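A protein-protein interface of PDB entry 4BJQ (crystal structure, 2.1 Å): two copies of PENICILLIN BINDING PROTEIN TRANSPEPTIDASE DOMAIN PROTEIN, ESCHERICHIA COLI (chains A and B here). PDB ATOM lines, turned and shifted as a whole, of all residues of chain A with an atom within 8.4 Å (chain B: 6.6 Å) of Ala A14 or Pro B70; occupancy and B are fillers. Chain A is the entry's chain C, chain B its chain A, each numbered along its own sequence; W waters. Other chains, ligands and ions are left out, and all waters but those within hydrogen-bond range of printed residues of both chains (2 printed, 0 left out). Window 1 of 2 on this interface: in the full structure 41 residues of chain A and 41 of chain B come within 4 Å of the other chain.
Printed residues of chain B within 4 Å of Trp A5: Gly B71, Ile B72 and His B73. Printed residues of chain B within 4 Å of Ala A6: Gly B71 and Ile B72. Of chain B, only Ala B14 (3.7 Å) and Pro B70 (3.7 Å) come within 4 Å of Ala A14. Arg A22 touches none of the printed residues of chain B. Of the printed residues of chain B, Pro A70 touches Ala B14 (3.5 Å). Asp B13 touches none of the printed residues of chain A. Pro B70 touches just these residues of chain A: Val A11 and Ala A14. Gly B71 touches just these residues of chain A: Trp A5, Ala A6, Asp A7, Glu A10 and Val A11. The nearest printed residue of chain B that does not touch Ala A14 is Gly B15 (5.8 Å). The nearest residue of chain A that does not touch Pro B70 is Glu A10 (4.6 Å). The nearest printed residue of chain B that does not touch Ala A6 is His B73 (5.0 Å).
The backbone carbonyl oxygen of Gly B71 is in hydrogen-bond range of the backbone NH of Asp A7 (2.7 Å). O of His B73 lies within hydrogen-bond range of N of Trp A5 (2.9 Å). OE1 of Glu A10 sits at hydrogen-bond distance from NE2 of His B73 (2.8 Å).
Water W1 lies within hydrogen-bond range of O of Gly A16 (2.6 Å) and NE1 of Trp B23 (2.9 Å). Water W2 bridges the backbone carbonyl oxygen (O) of Ala B14 (2.7 Å) and the backbone carbonyl oxygen (O) of Ala A14 (3.0 Å).
Ala A14 touches its own counterpart, Ala B14. Ala A14 touches Pro B70, and with the chains exchanged Pro A70 touches Ala B14. Val B19 touches its own counterpart, Val A19. Of the 15 pairs that touch across the chains among the printed residues, 4 have their exchanged pair printed and touching as well.
Printed residues of chain A that touch a printed residue of chain B: Trp A5, Ala A6, Asp A7, Glu A10, Val A11, Ala A14, Ile A17, Val A19 and Pro A70. Hydrophobic or aromatic side chains of chain A within 4 Å of the printed part of chain B: Trp A5, Ala A6, Val A11, Ala A14, Ile A17, Val A19 and Pro A70. Of the 12 printed residues of chain B, 7 touch a printed residue of chain A. Printed residues of chain B that touch a printed residue of chain A: Ala B14, Val B19, Trp B23, Pro B70, Gly B71, Ile B72 and His B73. Hydrophobic or aromatic side chains of chain B within 4 Å of the printed part of chain A: Ala B14, Val B19, Trp B23, Pro B70, Ile B72 and His B73.
The backbone NH of Lys A9 sits close to the side-chain carboxylate of Asp A7 (3.2 Å). OD1 of Asp A7 lies within hydrogen-bond range of N of Glu A10 (3.4 Å). O of Val A11 is in hydrogen-bond range of N of Gly A16 (3.0 Å).
Among the printed residues, pairs that only touch across the chains: Trp A5 with Gly B71 (3.7 Å), Trp A5 with Ile B72 (3.6 Å), Ala A6 with Gly B71 (3.2 Å), Ala A6 with Ile B72 (3.9 Å), Glu A10 with Gly B71 (3.5 Å), Val A11 with Pro B70 (3.4 Å), Val A11 with Gly B71 (3.9 Å), Ala A14 with Ala B14 (3.7 Å), Ala A14 with Pro B70 (3.7 Å), Ile A17 with Trp B23 (3.6 Å), Val A19 with Val B19 (3.5 Å) and Pro A70 with Ala B14 (3.5 Å).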
ATOM      1  N   TRP A   5      -2.165  25.458  13.887  1.00  0.00           N
ATOM      2  CA  TRP A   5      -3.309  26.342  14.029  1.00  0.00           C
ATOM      3  C   TRP A   5      -4.077  26.075  15.309  1.00  0.00           C
ATOM      4  O   TRP A   5      -3.972  24.998  15.910  1.00  0.00           O
ATOM      5  CB  TRP A   5      -4.223  26.300  12.785  1.00  0.00           C
ATOM      6  CG  TRP A   5      -5.339  25.261  12.747  1.00  0.00           C
ATOM      7  CD1 TRP A   5      -6.604  25.384  13.250  1.00  0.00           C
ATOM      8  CD2 TRP A   5      -5.285  23.975  12.118  1.00  0.00           C
ATOM      9  NE1 TRP A   5      -7.335  24.249  12.990  1.00  0.00           N
ATOM     10  CE2 TRP A   5      -6.550  23.373  12.287  1.00  0.00           C
ATOM     11  CE3 TRP A   5      -4.286  23.277  11.421  1.00  0.00           C
ATOM     12  CZ2 TRP A   5      -6.842  22.100  11.798  1.00  0.00           C
ATOM     13  CZ3 TRP A   5      -4.576  22.015  10.942  1.00  0.00           C
ATOM     14  CH2 TRP A   5      -5.846  21.441  11.125  1.00  0.00           C
ATOM     15  N   ALA A   6      -4.818  27.094  15.728  1.00  0.00           N
ATOM     16  CA  ALA A   6      -5.705  26.987  16.858  1.00  0.00           C
ATOM     17  C   ALA A   6      -7.151  27.043  16.367  1.00  0.00           C
ATOM     18  O   ALA A   6      -7.452  27.650  15.334  1.00  0.00           O
ATOM     19  CB  ALA A   6      -5.426  28.090  17.858  1.00  0.00           C
ATOM     20  N   ASP A   7      -8.029  26.370  17.100  1.00  0.00           N
ATOM     21  CA  ASP A   7      -9.467  26.457  16.908  1.00  0.00           C
ATOM     22  C   ASP A   7     -10.021  27.226  18.113  1.00  0.00           C
ATOM     23  O   ASP A   7     -10.249  26.626  19.165  1.00  0.00           O
ATOM     24  CB  ASP A   7     -10.056  25.044  16.829  1.00  0.00           C
ATOM     25  CG  ASP A   7     -11.591  25.031  16.739  1.00  0.00           C
ATOM     26  OD1 ASP A   7     -12.243  26.085  16.915  1.00  0.00           O
ATOM     27  OD2 ASP A   7     -12.148  23.937  16.506  1.00  0.00           O
ATOM     28  N   PRO A   8     -10.207  28.560  17.971  1.00  0.00           N
ATOM     29  CA  PRO A   8     -10.595  29.427  19.085  1.00  0.00           C
ATOM     30  C   PRO A   8     -11.842  28.996  19.845  1.00  0.00           C
ATOM     31  O   PRO A   8     -11.942  29.282  21.039  1.00  0.00           O
ATOM     32  CB  PRO A   8     -10.828  30.787  18.416  1.00  0.00           C
ATOM     33  CG  PRO A   8      -9.951  30.758  17.211  1.00  0.00           C
ATOM     34  CD  PRO A   8      -9.990  29.331  16.731  1.00  0.00           C
ATOM     35  N   LYS A   9     -12.788  28.346  19.163  1.00  0.00           N
ATOM     36  CA  LYS A   9     -14.013  27.830  19.797  1.00  0.00           C
ATOM     37  C   LYS A   9     -13.755  26.604  20.696  1.00  0.00           C
ATOM     38  O   LYS A   9     -14.299  26.524  21.797  1.00  0.00           O
ATOM     39  CB  LYS A   9     -15.081  27.512  18.735  1.00  0.00           C
ATOM     40  CG  LYS A   9     -16.436  27.098  19.302  1.00  0.00           C
ATOM     41  CD  LYS A   9     -17.424  26.706  18.193  1.00  0.00           C
ATOM     42  CE  LYS A   9     -18.366  25.589  18.637  1.00  0.00           C
ATOM     43  NZ  LYS A   9     -19.312  26.075  19.681  1.00  0.00           N
ATOM     44  N   GLU A  10     -12.938  25.658  20.228  1.00  0.00           N
ATOM     45  CA  GLU A  10     -12.510  24.512  21.039  1.00  0.00           C
ATOM     46  C   GLU A  10     -11.717  24.965  22.274  1.00  0.00           C
ATOM     47  O   GLU A  10     -11.857  24.385  23.360  1.00  0.00           O
ATOM     48  CB  GLU A  10     -11.646  23.542  20.218  1.00  0.00           C
ATOM     49  CG  GLU A  10     -12.408  22.451  19.479  1.00  0.00           C
ATOM     50  CD  GLU A  10     -11.505  21.523  18.642  1.00  0.00           C
ATOM     51  OE1 GLU A  10     -10.493  21.978  18.058  1.00  0.00           O
ATOM     52  OE2 GLU A  10     -11.822  20.320  18.553  1.00  0.00           O
ATOM     53  N   VAL A  11     -10.887  25.995  22.094  1.00  0.00           N
ATOM     54  CA  VAL A  11     -10.050  26.523  23.173  1.00  0.00           C
ATOM     55  C   VAL A  11     -10.926  27.173  24.254  1.00  0.00           C
ATOM     56  O   VAL A  11     -10.739  26.917  25.449  1.00  0.00           O
ATOM     57  CB  VAL A  11      -8.961  27.525  22.651  1.00  0.00           C
ATOM     58  CG1 VAL A  11      -8.194  28.171  23.811  1.00  0.00           C
ATOM     59  CG2 VAL A  11      -7.980  26.826  21.720  1.00  0.00           C
ATOM     60  N   HIS A  12     -11.870  28.013  23.826  1.00  0.00           N
ATOM     61  CA  HIS A  12     -12.864  28.591  24.730  1.00  0.00           C
ATOM     62  C   HIS A  12     -13.695  27.504  25.432  1.00  0.00           C
ATOM     63  O   HIS A  12     -13.821  27.523  26.657  1.00  0.00           O
ATOM     64  CB  HIS A  12     -13.776  29.565  23.981  1.00  0.00           C
ATOM     65  CG  HIS A  12     -14.894  30.104  24.817  1.00  0.00           C
ATOM     66  ND1 HIS A  12     -16.116  29.474  24.922  1.00  0.00           N
ATOM     67  CD2 HIS A  12     -14.969  31.202  25.608  1.00  0.00           C
ATOM     68  CE1 HIS A  12     -16.899  30.166  25.733  1.00  0.00           C
ATOM     69  NE2 HIS A  12     -16.225  31.217  26.165  1.00  0.00           N
ATOM     70  N   ASP A  13     -14.249  26.563  24.661  1.00  0.00           N
ATOM     71  CA  ASP A  13     -15.078  25.473  25.220  1.00  0.00           C
ATOM     72  C   ASP A  13     -14.357  24.624  26.263  1.00  0.00           C
ATOM     73  O   ASP A  13     -14.993  23.987  27.100  1.00  0.00           O
ATOM     74  CB  ASP A  13     -15.582  24.540  24.117  1.00  0.00           C
ATOM     75  CG  ASP A  13     -16.755  25.103  23.347  1.00  0.00           C
ATOM     76  OD1 ASP A  13     -17.244  26.217  23.657  1.00  0.00           O
ATOM     77  OD2 ASP A  13     -17.191  24.401  22.411  1.00  0.00           O
ATOM     78  N   ALA A  14     -13.030  24.596  26.194  1.00  0.00           N
ATOM     79  CA  ALA A  14     -12.248  23.801  27.120  1.00  0.00           C
ATOM     80  C   ALA A  14     -11.991  24.571  28.410  1.00  0.00           C
ATOM     81  O   ALA A  14     -11.404  24.035  29.353  1.00  0.00           O
ATOM     82  CB  ALA A  14     -10.955  23.366  26.481  1.00  0.00           C
ATOM     83  N   GLY A  15     -12.430  25.830  28.445  1.00  0.00           N
ATOM     84  CA  GLY A  15     -12.233  26.680  29.615  1.00  0.00           C
ATOM     85  C   GLY A  15     -11.287  27.844  29.395  1.00  0.00           C
ATOM     86  O   GLY A  15     -11.188  28.714  30.242  1.00  0.00           O
ATOM     87  N   GLY A  16     -10.578  27.855  28.268  1.00  0.00           N
ATOM     88  CA  GLY A  16      -9.652  28.952  27.929  1.00  0.00           C
ATOM     89  C   GLY A  16      -8.179  28.694  28.213  1.00  0.00           C
ATOM     90  O   GLY A  16      -7.827  27.742  28.925  1.00  0.00           O
ATOM     91  N   ILE A  17      -7.317  29.563  27.676  1.00  0.00           N
ATOM     92  CA  ILE A  17      -5.857  29.428  27.803  1.00  0.00           C
ATOM     93  C   ILE A  17      -5.347  29.718  29.222  1.00  0.00           C
ATOM     94  O   ILE A  17      -4.326  29.178  29.637  1.00  0.00           O
ATOM     95  CB  ILE A  17      -5.112  30.320  26.754  1.00  0.00           C
ATOM     96  CG1 ILE A  17      -5.097  29.634  25.388  1.00  0.00           C
ATOM     97  CG2 ILE A  17      -3.670  30.651  27.189  1.00  0.00           C
ATOM     98  CD1 ILE A  17      -4.727  30.548  24.225  1.00  0.00           C
ATOM     99  N   VAL A  19      -6.921  28.994  32.030  1.00  0.00           N
ATOM    100  CA  VAL A  19      -7.707  28.152  32.930  1.00  0.00           C
ATOM    101  C   VAL A  19      -6.946  27.832  34.238  1.00  0.00           C
ATOM    102  O   VAL A  19      -7.555  27.748  35.312  1.00  0.00           O
ATOM    103  CB  VAL A  19      -8.201  26.879  32.182  1.00  0.00           C
ATOM    104  CG1 VAL A  19      -7.083  25.833  32.031  1.00  0.00           C
ATOM    105  CG2 VAL A  19      -9.435  26.295  32.829  1.00  0.00           C
ATOM    106  N   GLY A  20      -5.619  27.712  34.145  1.00  0.00           N
ATOM    107  CA  GLY A  20      -4.759  27.379  35.285  1.00  0.00           C
ATOM    108  C   GLY A  20      -4.878  28.314  36.472  1.00  0.00           C
ATOM    109  O   GLY A  20      -4.807  27.887  37.637  1.00  0.00           O
ATOM    110  N   ARG A  22      -7.588  29.875  37.189  1.00  0.00           N
ATOM    111  CA  ARG A  22      -8.874  29.541  37.772  1.00  0.00           C
ATOM    112  C   ARG A  22      -8.906  28.174  38.500  1.00  0.00           C
ATOM    113  O   ARG A  22      -9.609  28.042  39.497  1.00  0.00           O
ATOM    114  CB  ARG A  22      -9.998  29.748  36.744  1.00  0.00           C
ATOM    115  CG  ARG A  22      -9.824  31.093  36.001  1.00  0.00           C
ATOM    116  CD  ARG A  22     -11.069  31.583  35.282  1.00  0.00           C
ATOM    117  NE  ARG A  22     -11.741  30.534  34.512  1.00  0.00           N
ATOM    118  CZ  ARG A  22     -11.448  30.195  33.259  1.00  0.00           C
ATOM    119  NH1 ARG A  22     -10.476  30.818  32.600  1.00  0.00           N
ATOM    120  NH2 ARG A  22     -12.137  29.216  32.669  1.00  0.00           N
ATOM    121  N   TRP A  23      -8.127  27.182  38.060  1.00  0.00           N
ATOM    122  CA  TRP A  23      -7.984  25.942  38.869  1.00  0.00           C
ATOM    123  C   TRP A  23      -7.357  26.223  40.248  1.00  0.00           C
ATOM    124  O   TRP A  23      -7.697  25.571  41.250  1.00  0.00           O
ATOM    125  CB  TRP A  23      -7.159  24.867  38.164  1.00  0.00           C
ATOM    126  CG  TRP A  23      -7.876  24.117  37.099  1.00  0.00           C
ATOM    127  CD1 TRP A  23      -7.602  24.140  35.760  1.00  0.00           C
ATOM    128  CD2 TRP A  23      -8.981  23.207  37.269  1.00  0.00           C
ATOM    129  NE1 TRP A  23      -8.462  23.307  35.085  1.00  0.00           N
ATOM    130  CE2 TRP A  23      -9.317  22.719  35.985  1.00  0.00           C
ATOM    131  CE3 TRP A  23      -9.715  22.756  38.383  1.00  0.00           C
ATOM    132  CZ2 TRP A  23     -10.366  21.800  35.777  1.00  0.00           C
ATOM    133  CZ3 TRP A  23     -10.756  21.833  38.178  1.00  0.00           C
ATOM    134  CH2 TRP A  23     -11.072  21.377  36.886  1.00  0.00           C
ATOM    135  N   LEU A  67     -16.130  30.520  37.747  1.00  0.00           N
ATOM    136  CA  LEU A  67     -14.799  30.086  37.283  1.00  0.00           C
ATOM    137  C   LEU A  67     -14.845  29.350  35.927  1.00  0.00           C
ATOM    138  O   LEU A  67     -13.810  29.189  35.259  1.00  0.00           O
ATOM    139  CB  LEU A  67     -14.122  29.200  38.332  1.00  0.00           C
ATOM    140  CG  LEU A  67     -13.721  29.816  39.676  1.00  0.00           C
ATOM    141  CD1 LEU A  67     -13.011  28.766  40.524  1.00  0.00           C
ATOM    142  CD2 LEU A  67     -12.830  31.069  39.496  1.00  0.00           C
ATOM    143  N   LYS A  68     -16.044  28.912  35.540  1.00  0.00           N
ATOM    144  CA  LYS A  68     -16.301  28.251  34.259  1.00  0.00           C
ATOM    145  C   LYS A  68     -15.322  27.128  33.924  1.00  0.00           C
ATOM    146  O   LYS A  68     -14.816  27.010  32.794  1.00  0.00           O
ATOM    147  CB  LYS A  68     -16.451  29.277  33.134  1.00  0.00           C
ATOM    148  CG  LYS A  68     -17.720  30.120  33.325  1.00  0.00           C
ATOM    149  CD  LYS A  68     -18.352  30.550  32.016  1.00  0.00           C
ATOM    150  CE  LYS A  68     -19.774  31.083  32.249  1.00  0.00           C
ATOM    151  NZ  LYS A  68     -20.723  30.037  32.777  1.00  0.00           N
ATOM    152  N   LEU A  69     -15.062  26.304  34.930  1.00  0.00           N
ATOM    153  CA  LEU A  69     -14.082  25.235  34.821  1.00  0.00           C
ATOM    154  C   LEU A  69     -14.693  24.037  34.124  1.00  0.00           C
ATOM    155  O   LEU A  69     -15.839  23.692  34.385  1.00  0.00           O
ATOM    156  CB  LEU A  69     -13.537  24.844  36.205  1.00  0.00           C
ATOM    157  CG  LEU A  69     -12.565  25.867  36.831  1.00  0.00           C
ATOM    158  CD1 LEU A  69     -12.130  25.472  38.252  1.00  0.00           C
ATOM    159  CD2 LEU A  69     -11.347  26.102  35.961  1.00  0.00           C
ATOM    160  N   PRO A  70     -13.935  23.405  33.220  1.00  0.00           N
ATOM    161  CA  PRO A  70     -14.488  22.208  32.594  1.00  0.00           C
ATOM    162  C   PRO A  70     -14.620  21.076  33.608  1.00  0.00           C
ATOM    163  O   PRO A  70     -13.720  20.884  34.438  1.00  0.00           O
ATOM    164  CB  PRO A  70     -13.446  21.855  31.535  1.00  0.00           C
ATOM    165  CG  PRO A  70     -12.142  22.401  32.086  1.00  0.00           C
ATOM    166  CD  PRO A  70     -12.557  23.686  32.775  1.00  0.00           C
ATOM    167  N   GLY A  71     -15.744  20.360  33.540  1.00  0.00           N
ATOM    168  CA  GLY A  71     -15.978  19.180  34.360  1.00  0.00           C
ATOM    169  C   GLY A  71     -16.332  19.427  35.821  1.00  0.00           C
ATOM    170  O   GLY A  71     -16.334  18.486  36.617  1.00  0.00           O
ATOM    171  N   ASP B  13     -10.709  15.457  29.143  1.00  0.00           N
ATOM    172  CA  ASP B  13     -11.067  15.761  27.754  1.00  0.00           C
ATOM    173  C   ASP B  13     -10.858  17.245  27.391  1.00  0.00           C
ATOM    174  O   ASP B  13     -10.772  17.598  26.216  1.00  0.00           O
ATOM    175  CB  ASP B  13     -12.521  15.346  27.455  1.00  0.00           C
ATOM    176  CG  ASP B  13     -12.751  13.827  27.554  1.00  0.00           C
ATOM    177  OD1 ASP B  13     -11.781  13.035  27.509  1.00  0.00           O
ATOM    178  OD2 ASP B  13     -13.925  13.418  27.667  1.00  0.00           O
ATOM    179  N   ALA B  14     -10.785  18.106  28.401  1.00  0.00           N
ATOM    180  CA  ALA B  14     -10.479  19.518  28.199  1.00  0.00           C
ATOM    181  C   ALA B  14      -8.966  19.797  28.314  1.00  0.00           C
ATOM    182  O   ALA B  14      -8.521  20.965  28.261  1.00  0.00           O
ATOM    183  CB  ALA B  14     -11.258  20.361  29.191  1.00  0.00           C
ATOM    184  N   GLY B  15      -8.189  18.728  28.496  1.00  0.00           N
ATOM    185  CA  GLY B  15      -6.739  18.831  28.529  1.00  0.00           C
ATOM    186  C   GLY B  15      -6.035  18.514  29.842  1.00  0.00           C
ATOM    187  O   GLY B  15      -4.794  18.505  29.889  1.00  0.00           O
ATOM    188  N   VAL B  19      -3.164  21.635  32.474  1.00  0.00           N
ATOM    189  CA  VAL B  19      -3.005  22.043  31.065  1.00  0.00           C
ATOM    190  C   VAL B  19      -2.338  23.420  30.907  1.00  0.00           C
ATOM    191  O   VAL B  19      -1.692  23.687  29.891  1.00  0.00           O
ATOM    192  CB  VAL B  19      -4.360  21.988  30.306  1.00  0.00           C
ATOM    193  CG1 VAL B  19      -5.280  23.139  30.708  1.00  0.00           C
ATOM    194  CG2 VAL B  19      -4.145  21.951  28.802  1.00  0.00           C
ATOM    195  N   TRP B  23       0.270  25.028  28.058  1.00  0.00           N
ATOM    196  CA  TRP B  23       0.101  26.284  27.311  1.00  0.00           C
ATOM    197  C   TRP B  23       1.375  27.121  27.354  1.00  0.00           C
ATOM    198  O   TRP B  23       1.826  27.614  26.319  1.00  0.00           O
ATOM    199  CB  TRP B  23      -1.094  27.104  27.814  1.00  0.00           C
ATOM    200  CG  TRP B  23      -2.430  26.555  27.354  1.00  0.00           C
ATOM    201  CD1 TRP B  23      -3.416  26.036  28.149  1.00  0.00           C
ATOM    202  CD2 TRP B  23      -2.913  26.452  25.997  1.00  0.00           C
ATOM    203  NE1 TRP B  23      -4.480  25.634  27.382  1.00  0.00           N
ATOM    204  CE2 TRP B  23      -4.200  25.865  26.059  1.00  0.00           C
ATOM    205  CE3 TRP B  23      -2.384  26.796  24.740  1.00  0.00           C
ATOM    206  CZ2 TRP B  23      -4.979  25.625  24.909  1.00  0.00           C
ATOM    207  CZ3 TRP B  23      -3.151  26.563  23.602  1.00  0.00           C
ATOM    208  CH2 TRP B  23      -4.440  25.970  23.694  1.00  0.00           C
ATOM    209  N   LEU B  67       2.026  17.781  23.453  1.00  0.00           N
ATOM    210  CA  LEU B  67       1.405  18.598  24.508  1.00  0.00           C
ATOM    211  C   LEU B  67      -0.117  18.343  24.625  1.00  0.00           C
ATOM    212  O   LEU B  67      -0.724  18.638  25.669  1.00  0.00           O
ATOM    213  CB  LEU B  67       1.668  20.099  24.276  1.00  0.00           C
ATOM    214  CG  LEU B  67       3.108  20.638  24.354  1.00  0.00           C
ATOM    215  CD1 LEU B  67       3.172  22.079  23.889  1.00  0.00           C
ATOM    216  CD2 LEU B  67       3.715  20.503  25.756  1.00  0.00           C
ATOM    217  N   LYS B  68      -0.718  17.809  23.556  1.00  0.00           N
ATOM    218  CA  LYS B  68      -2.137  17.407  23.541  1.00  0.00           C
ATOM    219  C   LYS B  68      -3.029  18.541  24.036  1.00  0.00           C
ATOM    220  O   LYS B  68      -3.848  18.360  24.938  1.00  0.00           O
ATOM    221  CB  LYS B  68      -2.364  16.121  24.363  1.00  0.00           C
ATOM    222  CG  LYS B  68      -1.574  14.900  23.867  1.00  0.00           C
ATOM    223  CD  LYS B  68      -2.245  13.567  24.256  1.00  0.00           C
ATOM    224  CE  LYS B  68      -2.194  13.316  25.761  1.00  0.00           C
ATOM    225  NZ  LYS B  68      -3.195  12.278  26.229  1.00  0.00           N
ATOM    226  N   LEU B  69      -2.838  19.724  23.454  1.00  0.00           N
ATOM    227  CA  LEU B  69      -3.539  20.914  23.900  1.00  0.00           C
ATOM    228  C   LEU B  69      -4.884  21.039  23.174  1.00  0.00           C
ATOM    229  O   LEU B  69      -4.959  20.888  21.946  1.00  0.00           O
ATOM    230  CB  LEU B  69      -2.663  22.163  23.675  1.00  0.00           C
ATOM    231  CG  LEU B  69      -1.503  22.472  24.652  1.00  0.00           C
ATOM    232  CD1 LEU B  69      -0.533  23.455  24.050  1.00  0.00           C
ATOM    233  CD2 LEU B  69      -1.978  23.013  26.012  1.00  0.00           C
ATOM    234  N   PRO B  70      -5.951  21.337  23.927  1.00  0.00           N
ATOM    235  CA  PRO B  70      -7.286  21.465  23.324  1.00  0.00           C
ATOM    236  C   PRO B  70      -7.306  22.600  22.298  1.00  0.00           C
ATOM    237  O   PRO B  70      -6.797  23.708  22.568  1.00  0.00           O
ATOM    238  CB  PRO B  70      -8.187  21.800  24.529  1.00  0.00           C
ATOM    239  CG  PRO B  70      -7.253  22.476  25.501  1.00  0.00           C
ATOM    240  CD  PRO B  70      -5.932  21.769  25.342  1.00  0.00           C
ATOM    241  N   GLY B  71      -7.853  22.305  21.122  1.00  0.00           N
ATOM    242  CA  GLY B  71      -7.963  23.273  20.036  1.00  0.00           C
ATOM    243  C   GLY B  71      -6.710  23.490  19.219  1.00  0.00           C
ATOM    244  O   GLY B  71      -6.702  24.311  18.302  1.00  0.00           O
ATOM    245  N   ILE B  72      -5.640  22.774  19.539  1.00  0.00           N
ATOM    246  CA  ILE B  72      -4.393  22.933  18.794  1.00  0.00           C
ATOM    247  C   ILE B  72      -4.285  21.831  17.761  1.00  0.00           C
ATOM    248  O   ILE B  72      -4.481  20.672  18.073  1.00  0.00           O
ATOM    249  CB  ILE B  72      -3.146  22.982  19.721  1.00  0.00           C
ATOM    250  CG1 ILE B  72      -3.217  24.202  20.642  1.00  0.00           C
ATOM    251  CG2 ILE B  72      -1.831  23.000  18.899  1.00  0.00           C
ATOM    252  CD1 ILE B  72      -3.340  25.534  19.906  1.00  0.00           C
ATOM    253  N   HIS B  73      -3.998  22.206  16.523  1.00  0.00           N
ATOM    254  CA  HIS B  73      -3.938  21.245  15.432  1.00  0.00           C
ATOM    255  C   HIS B  73      -2.766  21.526  14.508  1.00  0.00           C
ATOM    256  O   HIS B  73      -2.253  22.657  14.440  1.00  0.00           O
ATOM    257  CB  HIS B  73      -5.228  21.289  14.606  1.00  0.00           C
ATOM    258  CG  HIS B  73      -6.470  21.050  15.404  1.00  0.00           C
ATOM    259  ND1 HIS B  73      -7.028  19.798  15.553  1.00  0.00           N
ATOM    260  CD2 HIS B  73      -7.268  21.903  16.091  1.00  0.00           C
ATOM    261  CE1 HIS B  73      -8.109  19.886  16.306  1.00  0.00           C
ATOM    262  NE2 HIS B  73      -8.277  21.151  16.644  1.00  0.00           N
HETATM  263  O   HOH W   1      -7.167  25.337  28.352  1.00  0.00           O
HETATM  264  O   HOH W   2      -8.603  23.178  29.839  1.00  0.00           O
